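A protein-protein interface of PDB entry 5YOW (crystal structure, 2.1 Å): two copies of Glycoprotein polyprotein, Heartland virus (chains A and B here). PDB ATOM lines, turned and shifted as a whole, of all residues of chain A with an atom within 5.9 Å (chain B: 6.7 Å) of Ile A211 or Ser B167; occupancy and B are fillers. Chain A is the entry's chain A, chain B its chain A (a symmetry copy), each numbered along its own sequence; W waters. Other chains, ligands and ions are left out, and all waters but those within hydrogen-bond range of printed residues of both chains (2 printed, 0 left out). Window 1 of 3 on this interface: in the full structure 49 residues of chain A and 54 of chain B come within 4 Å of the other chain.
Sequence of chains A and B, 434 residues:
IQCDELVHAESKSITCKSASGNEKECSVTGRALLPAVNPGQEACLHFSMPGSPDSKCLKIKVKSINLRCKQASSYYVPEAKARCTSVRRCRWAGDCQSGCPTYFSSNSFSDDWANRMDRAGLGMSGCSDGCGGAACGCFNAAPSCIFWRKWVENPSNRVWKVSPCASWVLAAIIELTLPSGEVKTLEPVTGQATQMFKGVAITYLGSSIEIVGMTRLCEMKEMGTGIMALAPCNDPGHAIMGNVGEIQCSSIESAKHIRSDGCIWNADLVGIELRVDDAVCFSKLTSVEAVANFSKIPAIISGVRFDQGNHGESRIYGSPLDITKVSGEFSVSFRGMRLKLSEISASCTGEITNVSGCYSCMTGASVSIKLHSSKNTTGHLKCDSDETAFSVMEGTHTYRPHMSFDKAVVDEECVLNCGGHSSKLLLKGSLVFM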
ATOM      1  N   LEU A  67     -14.368  26.221 -10.375  1.00  0.00           N
ATOM      2  CA  LEU A  67     -14.679  27.632 -10.506  1.00  0.00           C
ATOM      3  C   LEU A  67     -13.636  28.449  -9.745  1.00  0.00           C
ATOM      4  O   LEU A  67     -13.494  28.286  -8.527  1.00  0.00           O
ATOM      5  CB  LEU A  67     -16.077  27.895  -9.948  1.00  0.00           C
ATOM      6  CG  LEU A  67     -17.250  27.229 -10.673  1.00  0.00           C
ATOM      7  CD1 LEU A  67     -18.489  27.215  -9.793  1.00  0.00           C
ATOM      8  CD2 LEU A  67     -17.531  28.030 -11.915  1.00  0.00           C
ATOM      9  N   ILE A 209     -20.294  24.598 -18.331  1.00  0.00           N
ATOM     10  CA  ILE A 209     -20.990  24.402 -17.060  1.00  0.00           C
ATOM     11  C   ILE A 209     -22.456  24.741 -17.257  1.00  0.00           C
ATOM     12  O   ILE A 209     -22.801  25.628 -18.044  1.00  0.00           O
ATOM     13  CB  ILE A 209     -20.369  25.227 -15.910  1.00  0.00           C
ATOM     14  CG1 ILE A 209     -21.063  24.928 -14.589  1.00  0.00           C
ATOM     15  CG2 ILE A 209     -20.495  26.694 -16.173  1.00  0.00           C
ATOM     16  CD1 ILE A 209     -20.240  25.370 -13.396  1.00  0.00           C
ATOM     17  N   GLU A 210     -23.313  23.990 -16.569  1.00  0.00           N
ATOM     18  CA  GLU A 210     -24.754  24.134 -16.650  1.00  0.00           C
ATOM     19  C   GLU A 210     -25.336  24.992 -15.519  1.00  0.00           C
ATOM     20  O   GLU A 210     -26.558  25.012 -15.342  1.00  0.00           O
ATOM     21  CB  GLU A 210     -25.385  22.751 -16.652  1.00  0.00           C
ATOM     22  CG  GLU A 210     -24.924  21.878 -17.833  1.00  0.00           C
ATOM     23  CD  GLU A 210     -25.929  20.795 -18.151  1.00  0.00           C
ATOM     24  OE1 GLU A 210     -25.591  19.802 -18.794  1.00  0.00           O
ATOM     25  OE2 GLU A 210     -27.098  20.961 -17.736  1.00  0.00           O
ATOM     26  N   ILE A 211     -24.493  25.691 -14.760  1.00  0.00           N
ATOM     27  CA  ILE A 211     -24.913  26.519 -13.621  1.00  0.00           C
ATOM     28  C   ILE A 211     -24.814  27.980 -14.038  1.00  0.00           C
ATOM     29  O   ILE A 211     -23.733  28.448 -14.404  1.00  0.00           O
ATOM     30  CB  ILE A 211     -24.040  26.248 -12.385  1.00  0.00           C
ATOM     31  CG1 ILE A 211     -24.259  24.827 -11.859  1.00  0.00           C
ATOM     32  CG2 ILE A 211     -24.286  27.291 -11.282  1.00  0.00           C
ATOM     33  CD1 ILE A 211     -23.262  24.434 -10.762  1.00  0.00           C
ATOM     34  N   VAL A 212     -25.931  28.698 -13.961  1.00  0.00           N
ATOM     35  CA  VAL A 212     -26.083  30.043 -14.513  1.00  0.00           C
ATOM     36  C   VAL A 212     -26.217  31.059 -13.378  1.00  0.00           C
ATOM     37  O   VAL A 212     -26.989  30.849 -12.435  1.00  0.00           O
ATOM     38  CB  VAL A 212     -27.313  30.111 -15.434  1.00  0.00           C
ATOM     39  CG1 VAL A 212     -27.459  31.486 -16.084  1.00  0.00           C
ATOM     40  CG2 VAL A 212     -27.231  29.017 -16.469  1.00  0.00           C
ATOM     41  N   GLY A 213     -25.471  32.151 -13.469  1.00  0.00           N
ATOM     42  CA  GLY A 213     -25.693  33.318 -12.627  1.00  0.00           C
ATOM     43  C   GLY A 213     -25.644  33.150 -11.119  1.00  0.00           C
ATOM     44  O   GLY A 213     -26.616  33.477 -10.437  1.00  0.00           O
ATOM     45  N   MET A 214     -24.512  32.698 -10.587  1.00  0.00           N
ATOM     46  CA  MET A 214     -24.376  32.456  -9.157  1.00  0.00           C
ATOM     47  C   MET A 214     -24.483  33.751  -8.357  1.00  0.00           C
ATOM     48  O   MET A 214     -24.249  34.861  -8.854  1.00  0.00           O
ATOM     49  CB  MET A 214     -23.038  31.791  -8.842  1.00  0.00           C
ATOM     50  CG  MET A 214     -23.068  30.755  -7.711  1.00  0.00           C
ATOM     51  SD  MET A 214     -21.555  29.753  -7.700  1.00  0.00           S
ATOM     52  CE  MET A 214     -20.955  30.029  -9.368  1.00  0.00           C
ATOM     53  N   THR A 215     -24.818  33.572  -7.082  1.00  0.00           N
ATOM     54  CA  THR A 215     -24.976  34.673  -6.144  1.00  0.00           C
ATOM     55  C   THR A 215     -23.622  35.286  -5.792  1.00  0.00           C
ATOM     56  O   THR A 215     -22.593  34.602  -5.727  1.00  0.00           O
ATOM     57  CB  THR A 215     -25.676  34.189  -4.868  1.00  0.00           C
ATOM     58  OG1 THR A 215     -26.073  35.314  -4.071  1.00  0.00           O
ATOM     59  CG2 THR A 215     -24.752  33.274  -4.060  1.00  0.00           C
ATOM     60  N   SER A 302     -25.161  25.866  -1.952  1.00  0.00           N
ATOM     61  CA  SER A 302     -26.092  25.631  -3.049  1.00  0.00           C
ATOM     62  C   SER A 302     -25.417  24.921  -4.215  1.00  0.00           C
ATOM     63  O   SER A 302     -25.172  25.526  -5.268  1.00  0.00           O
ATOM     64  CB  SER A 302     -26.701  26.962  -3.507  1.00  0.00           C
ATOM     65  OG  SER A 302     -27.245  27.687  -2.406  1.00  0.00           O
ATOM     66  N   GLY A 303     -25.035  23.668  -4.006  1.00  0.00           N
ATOM     67  CA  GLY A 303     -24.557  22.831  -5.085  1.00  0.00           C
ATOM     68  C   GLY A 303     -23.085  22.921  -5.421  1.00  0.00           C
ATOM     69  O   GLY A 303     -22.627  22.154  -6.272  1.00  0.00           O
ATOM     70  N   VAL A 304     -22.328  23.812  -4.777  1.00  0.00           N
ATOM     71  CA  VAL A 304     -20.911  24.006  -5.049  1.00  0.00           C
ATOM     72  C   VAL A 304     -20.138  23.946  -3.746  1.00  0.00           C
ATOM     73  O   VAL A 304     -20.481  24.638  -2.780  1.00  0.00           O
ATOM     74  CB  VAL A 304     -20.642  25.352  -5.744  1.00  0.00           C
ATOM     75  CG1 VAL A 304     -19.180  25.474  -6.080  1.00  0.00           C
ATOM     76  CG2 VAL A 304     -21.484  25.483  -7.000  1.00  0.00           C
ATOM     77  N   PRO A 320     -18.424  22.157  -8.431  1.00  0.00           N
ATOM     78  CA  PRO A 320     -19.823  21.729  -8.549  1.00  0.00           C
ATOM     79  C   PRO A 320     -20.001  20.333  -7.984  1.00  0.00           C
ATOM     80  O   PRO A 320     -19.242  19.409  -8.310  1.00  0.00           O
ATOM     81  CB  PRO A 320     -20.074  21.754 -10.058  1.00  0.00           C
ATOM     82  CG  PRO A 320     -19.007  22.674 -10.597  1.00  0.00           C
ATOM     83  CD  PRO A 320     -17.824  22.481  -9.729  1.00  0.00           C
ATOM     84  N   LYS A 325     -22.980  18.415 -14.172  1.00  0.00           N
ATOM     85  CA  LYS A 325     -23.263  19.789 -14.588  1.00  0.00           C
ATOM     86  C   LYS A 325     -22.022  20.547 -15.067  1.00  0.00           C
ATOM     87  O   LYS A 325     -22.107  21.759 -15.268  1.00  0.00           O
ATOM     88  CB  LYS A 325     -23.937  20.552 -13.448  1.00  0.00           C
ATOM     89  CG  LYS A 325     -25.297  19.924 -13.055  1.00  0.00           C
ATOM     90  CD  LYS A 325     -26.240  19.906 -14.280  1.00  0.00           C
ATOM     91  CE  LYS A 325     -27.640  19.345 -13.973  1.00  0.00           C
ATOM     92  NZ  LYS A 325     -28.394  19.101 -15.260  1.00  0.00           N
ATOM     93  N   ARG B  68     -33.661  25.936 -13.508  1.00  0.00           N
ATOM     94  CA  ARG B  68     -34.241  25.612 -12.205  1.00  0.00           C
ATOM     95  C   ARG B  68     -33.513  26.360 -11.103  1.00  0.00           C
ATOM     96  O   ARG B  68     -32.280  26.405 -11.072  1.00  0.00           O
ATOM     97  CB  ARG B  68     -34.172  24.117 -11.888  1.00  0.00           C
ATOM     98  CG  ARG B  68     -34.975  23.240 -12.805  1.00  0.00           C
ATOM     99  CD  ARG B  68     -34.924  21.776 -12.374  1.00  0.00           C
ATOM    100  NE  ARG B  68     -35.835  20.971 -13.187  1.00  0.00           N
ATOM    101  CZ  ARG B  68     -35.794  19.648 -13.287  1.00  0.00           C
ATOM    102  NH1 ARG B  68     -34.878  18.956 -12.624  1.00  0.00           N
ATOM    103  NH2 ARG B  68     -36.668  19.023 -14.059  1.00  0.00           N
ATOM    104  N   CYS B  69     -34.284  26.896 -10.166  1.00  0.00           N
ATOM    105  CA  CYS B  69     -33.745  27.733  -9.102  1.00  0.00           C
ATOM    106  C   CYS B  69     -33.054  26.854  -8.063  1.00  0.00           C
ATOM    107  O   CYS B  69     -33.675  25.953  -7.502  1.00  0.00           O
ATOM    108  CB  CYS B  69     -34.874  28.565  -8.482  1.00  0.00           C
ATOM    109  SG  CYS B  69     -34.503  29.319  -6.882  1.00  0.00           S
ATOM    110  N   LYS B  70     -31.767  27.097  -7.824  1.00  0.00           N
ATOM    111  CA  LYS B  70     -31.038  26.450  -6.740  1.00  0.00           C
ATOM    112  C   LYS B  70     -31.016  27.428  -5.569  1.00  0.00           C
ATOM    113  O   LYS B  70     -30.349  28.466  -5.629  1.00  0.00           O
ATOM    114  CB  LYS B  70     -29.620  26.064  -7.162  1.00  0.00           C
ATOM    115  CG  LYS B  70     -29.055  24.880  -6.384  1.00  0.00           C
ATOM    116  CD  LYS B  70     -29.646  23.563  -6.892  1.00  0.00           C
ATOM    117  CE  LYS B  70     -28.929  22.341  -6.316  1.00  0.00           C
ATOM    118  NZ  LYS B  70     -28.965  22.291  -4.817  1.00  0.00           N
ATOM    119  N   GLN B  71     -31.732  27.088  -4.501  1.00  0.00           N
ATOM    120  CA  GLN B  71     -32.025  28.052  -3.445  1.00  0.00           C
ATOM    121  C   GLN B  71     -30.854  28.275  -2.483  1.00  0.00           C
ATOM    122  O   GLN B  71     -30.128  27.339  -2.126  1.00  0.00           O
ATOM    123  CB  GLN B  71     -33.240  27.588  -2.650  1.00  0.00           C
ATOM    124  CG  GLN B  71     -34.505  27.395  -3.469  1.00  0.00           C
ATOM    125  CD  GLN B  71     -35.646  26.902  -2.597  1.00  0.00           C
ATOM    126  OE1 GLN B  71     -35.422  26.550  -1.438  1.00  0.00           O
ATOM    127  NE2 GLN B  71     -36.868  26.884  -3.134  1.00  0.00           N
ATOM    128  N   ALA B  72     -30.706  29.520  -2.031  1.00  0.00           N
ATOM    129  CA  ALA B  72     -29.995  29.802  -0.786  1.00  0.00           C
ATOM    130  C   ALA B  72     -30.874  29.377   0.401  1.00  0.00           C
ATOM    131  O   ALA B  72     -31.936  28.762   0.239  1.00  0.00           O
ATOM    132  CB  ALA B  72     -29.619  31.277  -0.696  1.00  0.00           C
ATOM    133  N   PRO B 164     -34.051  32.945  -1.745  1.00  0.00           N
ATOM    134  CA  PRO B 164     -33.183  33.481  -2.792  1.00  0.00           C
ATOM    135  C   PRO B 164     -32.729  32.346  -3.704  1.00  0.00           C
ATOM    136  O   PRO B 164     -32.540  31.209  -3.258  1.00  0.00           O
ATOM    137  CB  PRO B 164     -32.005  34.089  -2.015  1.00  0.00           C
ATOM    138  CG  PRO B 164     -32.497  34.224  -0.580  1.00  0.00           C
ATOM    139  CD  PRO B 164     -33.463  33.094  -0.401  1.00  0.00           C
ATOM    140  N   CYS B 165     -32.596  32.649  -4.994  1.00  0.00           N
ATOM    141  CA  CYS B 165     -32.046  31.680  -5.937  1.00  0.00           C
ATOM    142  C   CYS B 165     -30.546  31.942  -6.035  1.00  0.00           C
ATOM    143  O   CYS B 165     -30.117  32.909  -6.665  1.00  0.00           O
ATOM    144  CB  CYS B 165     -32.747  31.794  -7.288  1.00  0.00           C
ATOM    145  SG  CYS B 165     -34.505  31.337  -7.238  1.00  0.00           S
ATOM    146  N   ALA B 166     -29.742  31.104  -5.373  1.00  0.00           N
ATOM    147  CA  ALA B 166     -28.291  31.292  -5.400  1.00  0.00           C
ATOM    148  C   ALA B 166     -27.716  31.082  -6.795  1.00  0.00           C
ATOM    149  O   ALA B 166     -26.715  31.716  -7.157  1.00  0.00           O
ATOM    150  CB  ALA B 166     -27.610  30.351  -4.415  1.00  0.00           C
ATOM    151  N   SER B 167     -28.330  30.206  -7.587  1.00  0.00           N
ATOM    152  CA  SER B 167     -27.999  30.067  -8.997  1.00  0.00           C
ATOM    153  C   SER B 167     -29.134  29.316  -9.659  1.00  0.00           C
ATOM    154  O   SER B 167     -30.041  28.795  -8.999  1.00  0.00           O
ATOM    155  CB  SER B 167     -26.663  29.342  -9.205  1.00  0.00           C
ATOM    156  OG  SER B 167     -26.739  28.072  -8.593  1.00  0.00           O
ATOM    157  N   TRP B 168     -29.087  29.283 -10.974  1.00  0.00           N
ATOM    158  CA  TRP B 168     -30.036  28.524 -11.760  1.00  0.00           C
ATOM    159  C   TRP B 168     -29.269  27.435 -12.492  1.00  0.00           C
ATOM    160  O   TRP B 168     -28.128  27.650 -12.916  1.00  0.00           O
ATOM    161  CB  TRP B 168     -30.788  29.446 -12.726  1.00  0.00           C
ATOM    162  CG  TRP B 168     -31.518  30.555 -12.021  1.00  0.00           C
ATOM    163  CD1 TRP B 168     -30.973  31.686 -11.481  1.00  0.00           C
ATOM    164  CD2 TRP B 168     -32.930  30.630 -11.764  1.00  0.00           C
ATOM    165  NE1 TRP B 168     -31.955  32.463 -10.917  1.00  0.00           N
ATOM    166  CE2 TRP B 168     -33.166  31.849 -11.087  1.00  0.00           C
ATOM    167  CE3 TRP B 168     -34.016  29.801 -12.070  1.00  0.00           C
ATOM    168  CZ2 TRP B 168     -34.430  32.241 -10.681  1.00  0.00           C
ATOM    169  CZ3 TRP B 168     -35.278  30.187 -11.656  1.00  0.00           C
ATOM    170  CH2 TRP B 168     -35.474  31.402 -10.966  1.00  0.00           C
ATOM    171  N   VAL B 169     -29.870  26.256 -12.592  1.00  0.00           N
ATOM    172  CA  VAL B 169     -29.232  25.092 -13.188  1.00  0.00           C
ATOM    173  C   VAL B 169     -30.090  24.646 -14.366  1.00  0.00           C
ATOM    174  O   VAL B 169     -31.320  24.700 -14.293  1.00  0.00           O
ATOM    175  CB  VAL B 169     -29.060  23.951 -12.164  1.00  0.00           C
ATOM    176  CG1 VAL B 169     -28.260  22.814 -12.774  1.00  0.00           C
ATOM    177  CG2 VAL B 169     -28.336  24.469 -10.920  1.00  0.00           C
ATOM    178  N   LEU B 170     -29.443  24.248 -15.459  1.00  0.00           N
ATOM    179  CA  LEU B 170     -30.186  23.824 -16.640  1.00  0.00           C
ATOM    180  C   LEU B 170     -30.795  22.453 -16.392  1.00  0.00           C
ATOM    181  O   LEU B 170     -30.196  21.598 -15.733  1.00  0.00           O
ATOM    182  CB  LEU B 170     -29.272  23.777 -17.881  1.00  0.00           C
ATOM    183  CG  LEU B 170     -28.521  25.075 -18.275  1.00  0.00           C
ATOM    184  CD1 LEU B 170     -27.558  24.861 -19.434  1.00  0.00           C
ATOM    185  CD2 LEU B 170     -29.516  26.167 -18.655  1.00  0.00           C
ATOM    186  N   ILE B 209     -25.988  27.067 -22.383  1.00  0.00           N
ATOM    187  CA  ILE B 209     -26.795  28.283 -22.480  1.00  0.00           C
ATOM    188  C   ILE B 209     -25.869  29.456 -22.742  1.00  0.00           C
ATOM    189  O   ILE B 209     -24.729  29.481 -22.267  1.00  0.00           O
ATOM    190  CB  ILE B 209     -27.664  28.519 -21.223  1.00  0.00           C
ATOM    191  CG1 ILE B 209     -28.553  29.742 -21.398  1.00  0.00           C
ATOM    192  CG2 ILE B 209     -26.812  28.741 -20.015  1.00  0.00           C
ATOM    193  CD1 ILE B 209     -29.697  29.766 -20.405  1.00  0.00           C
HETATM  194  O   HOH W   1     -23.534  26.710 -20.588  1.00  0.00           O
HETATM  195  O   HOH W   2     -24.821  27.981  -6.230  1.00  0.00           O
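The backbone NH (N) of Ala B166 lies within hydrogen-bond range of the backbone carbonyl oxygen (O) of Lys B70, at 2.7 Å. The backbone NH of Lys B70 sits at hydrogen-bond distance from the backbone carbonyl oxygen of Ser B167 (2.7 Å). The backbone NH of Arg B68 lies within hydrogen-bond range of the backbone carbonyl oxygen of Val B169, at 2.8 Å. The side-chain sulfur (SG) of Cys B69 forms a disulfide with the side-chain sulfur (SG) of Cys B165 (2.0 Å). The backbone carbonyl oxygen (O) of Pro B164 sits at hydrogen-bond distance from the backbone NH (N) of Ala B72, at 2.8 Å. NZ of Lys A325 lies within salt-bridge range of OE2 of Glu A210.
Of the 13 printed residues of chain A, 8 touch a printed residue of chain B. Hydrophobic or aromatic side chains of chain A that line the printed part of chain B: Ile A211, Val A212 and Met A214. Printed residues of chain B that touch a printed residue of chain A: Gln B71, Ala B72, Ala B166, Ser B167, Trp B168, Val B169, Leu B170 and Ile B209. Hydrophobic or aromatic side chains of chain B that line the printed part of chain A: Ala B166, Val B169, Leu B170 and Ile B209. Along chain B the printed residues that touch a printed residue of chain A span positions 71 to 209. Among the printed residues, 18 pairs touch across the chains. Among the printed residues, no Asp or Glu carboxylate lies within 4 Å of a Lys or Arg side-chain nitrogen of the other chain.
1 position is printed for both chains. Of the 18 pairs that touch across the chains among the printed residues, none has its exchanged pair printed and touching as well.
Ile A211 touches just these residues of chain B: Ser B167 and Trp B168. Ser B167 touches just these residues of chain A: Ile A211, Val A212, Gly A213 and Met A214. Of the printed residues of chain B, Thr A215 touches Ala B166. Printed residues of chain B within 4 Å of Met A214: Ala B166 (3.2 Å) and Ser B167 (3.9 Å). Of the printed residues of chain B, Val A212 touches Ser B167, Trp B168 and Ile B209. Val A304 touches none of the printed residues of chain B. The nearest residue of chain B that does not touch Ile A211 is Val B169 (4.2 Å). The nearest residue of chain A that does not touch Ser B167 is Ser A302 (4.5 Å).
Water W2 bridges O of Ser A302 (2.7 Å) and OG of Ser B167 (3.0 Å). Water W1 lies within hydrogen-bond range of the backbone carbonyl oxygen of Ile A209 (2.9 Å) and the backbone NH of Ile B209 (3.1 Å).
The backbone carbonyl oxygen (O) of Leu B170 sits at hydrogen-bond distance from the side-chain amino group (NZ) of Lys A325 (3.1 Å). The backbone carbonyl oxygen (O) of Glu A210 is in hydrogen-bond range of the backbone NH (N) of Leu B170 (3.0 Å). The backbone carbonyl oxygen (O) of Ala B166 is in hydrogen-bond range of the backbone NH (N) of Thr A215. N of Val A212 lies within hydrogen-bond range of O of Trp B168, 2.6 Å away. The side-chain hydroxyl (OG) of Ser A302 is in hydrogen-bond range of the backbone carbonyl oxygen (O) of Gln B71, at 2.9 Å.
Glu A210 touches Trp B168. Trp B168 touches Ile A211. O of Val A212 touches CB of Ser B167, 3.6 Å away. CG2 of Val A212 touches CG2 of Ile B209, at 3.6 Å. Ala B166 touches Gly A213. CA of Ser B167 touches O of Gly A213 (3.95 Å). CB of Ser B167 touches CA of Met A214, 3.9 Å away. CA of Ala B72 touches OG of Ser A302 (3.8 Å). Ser A302 touches Ala B166 (OG to CB, 3.4 Å). CE of Lys A325 touches CG1 of Val B169, 3.7 Å away.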
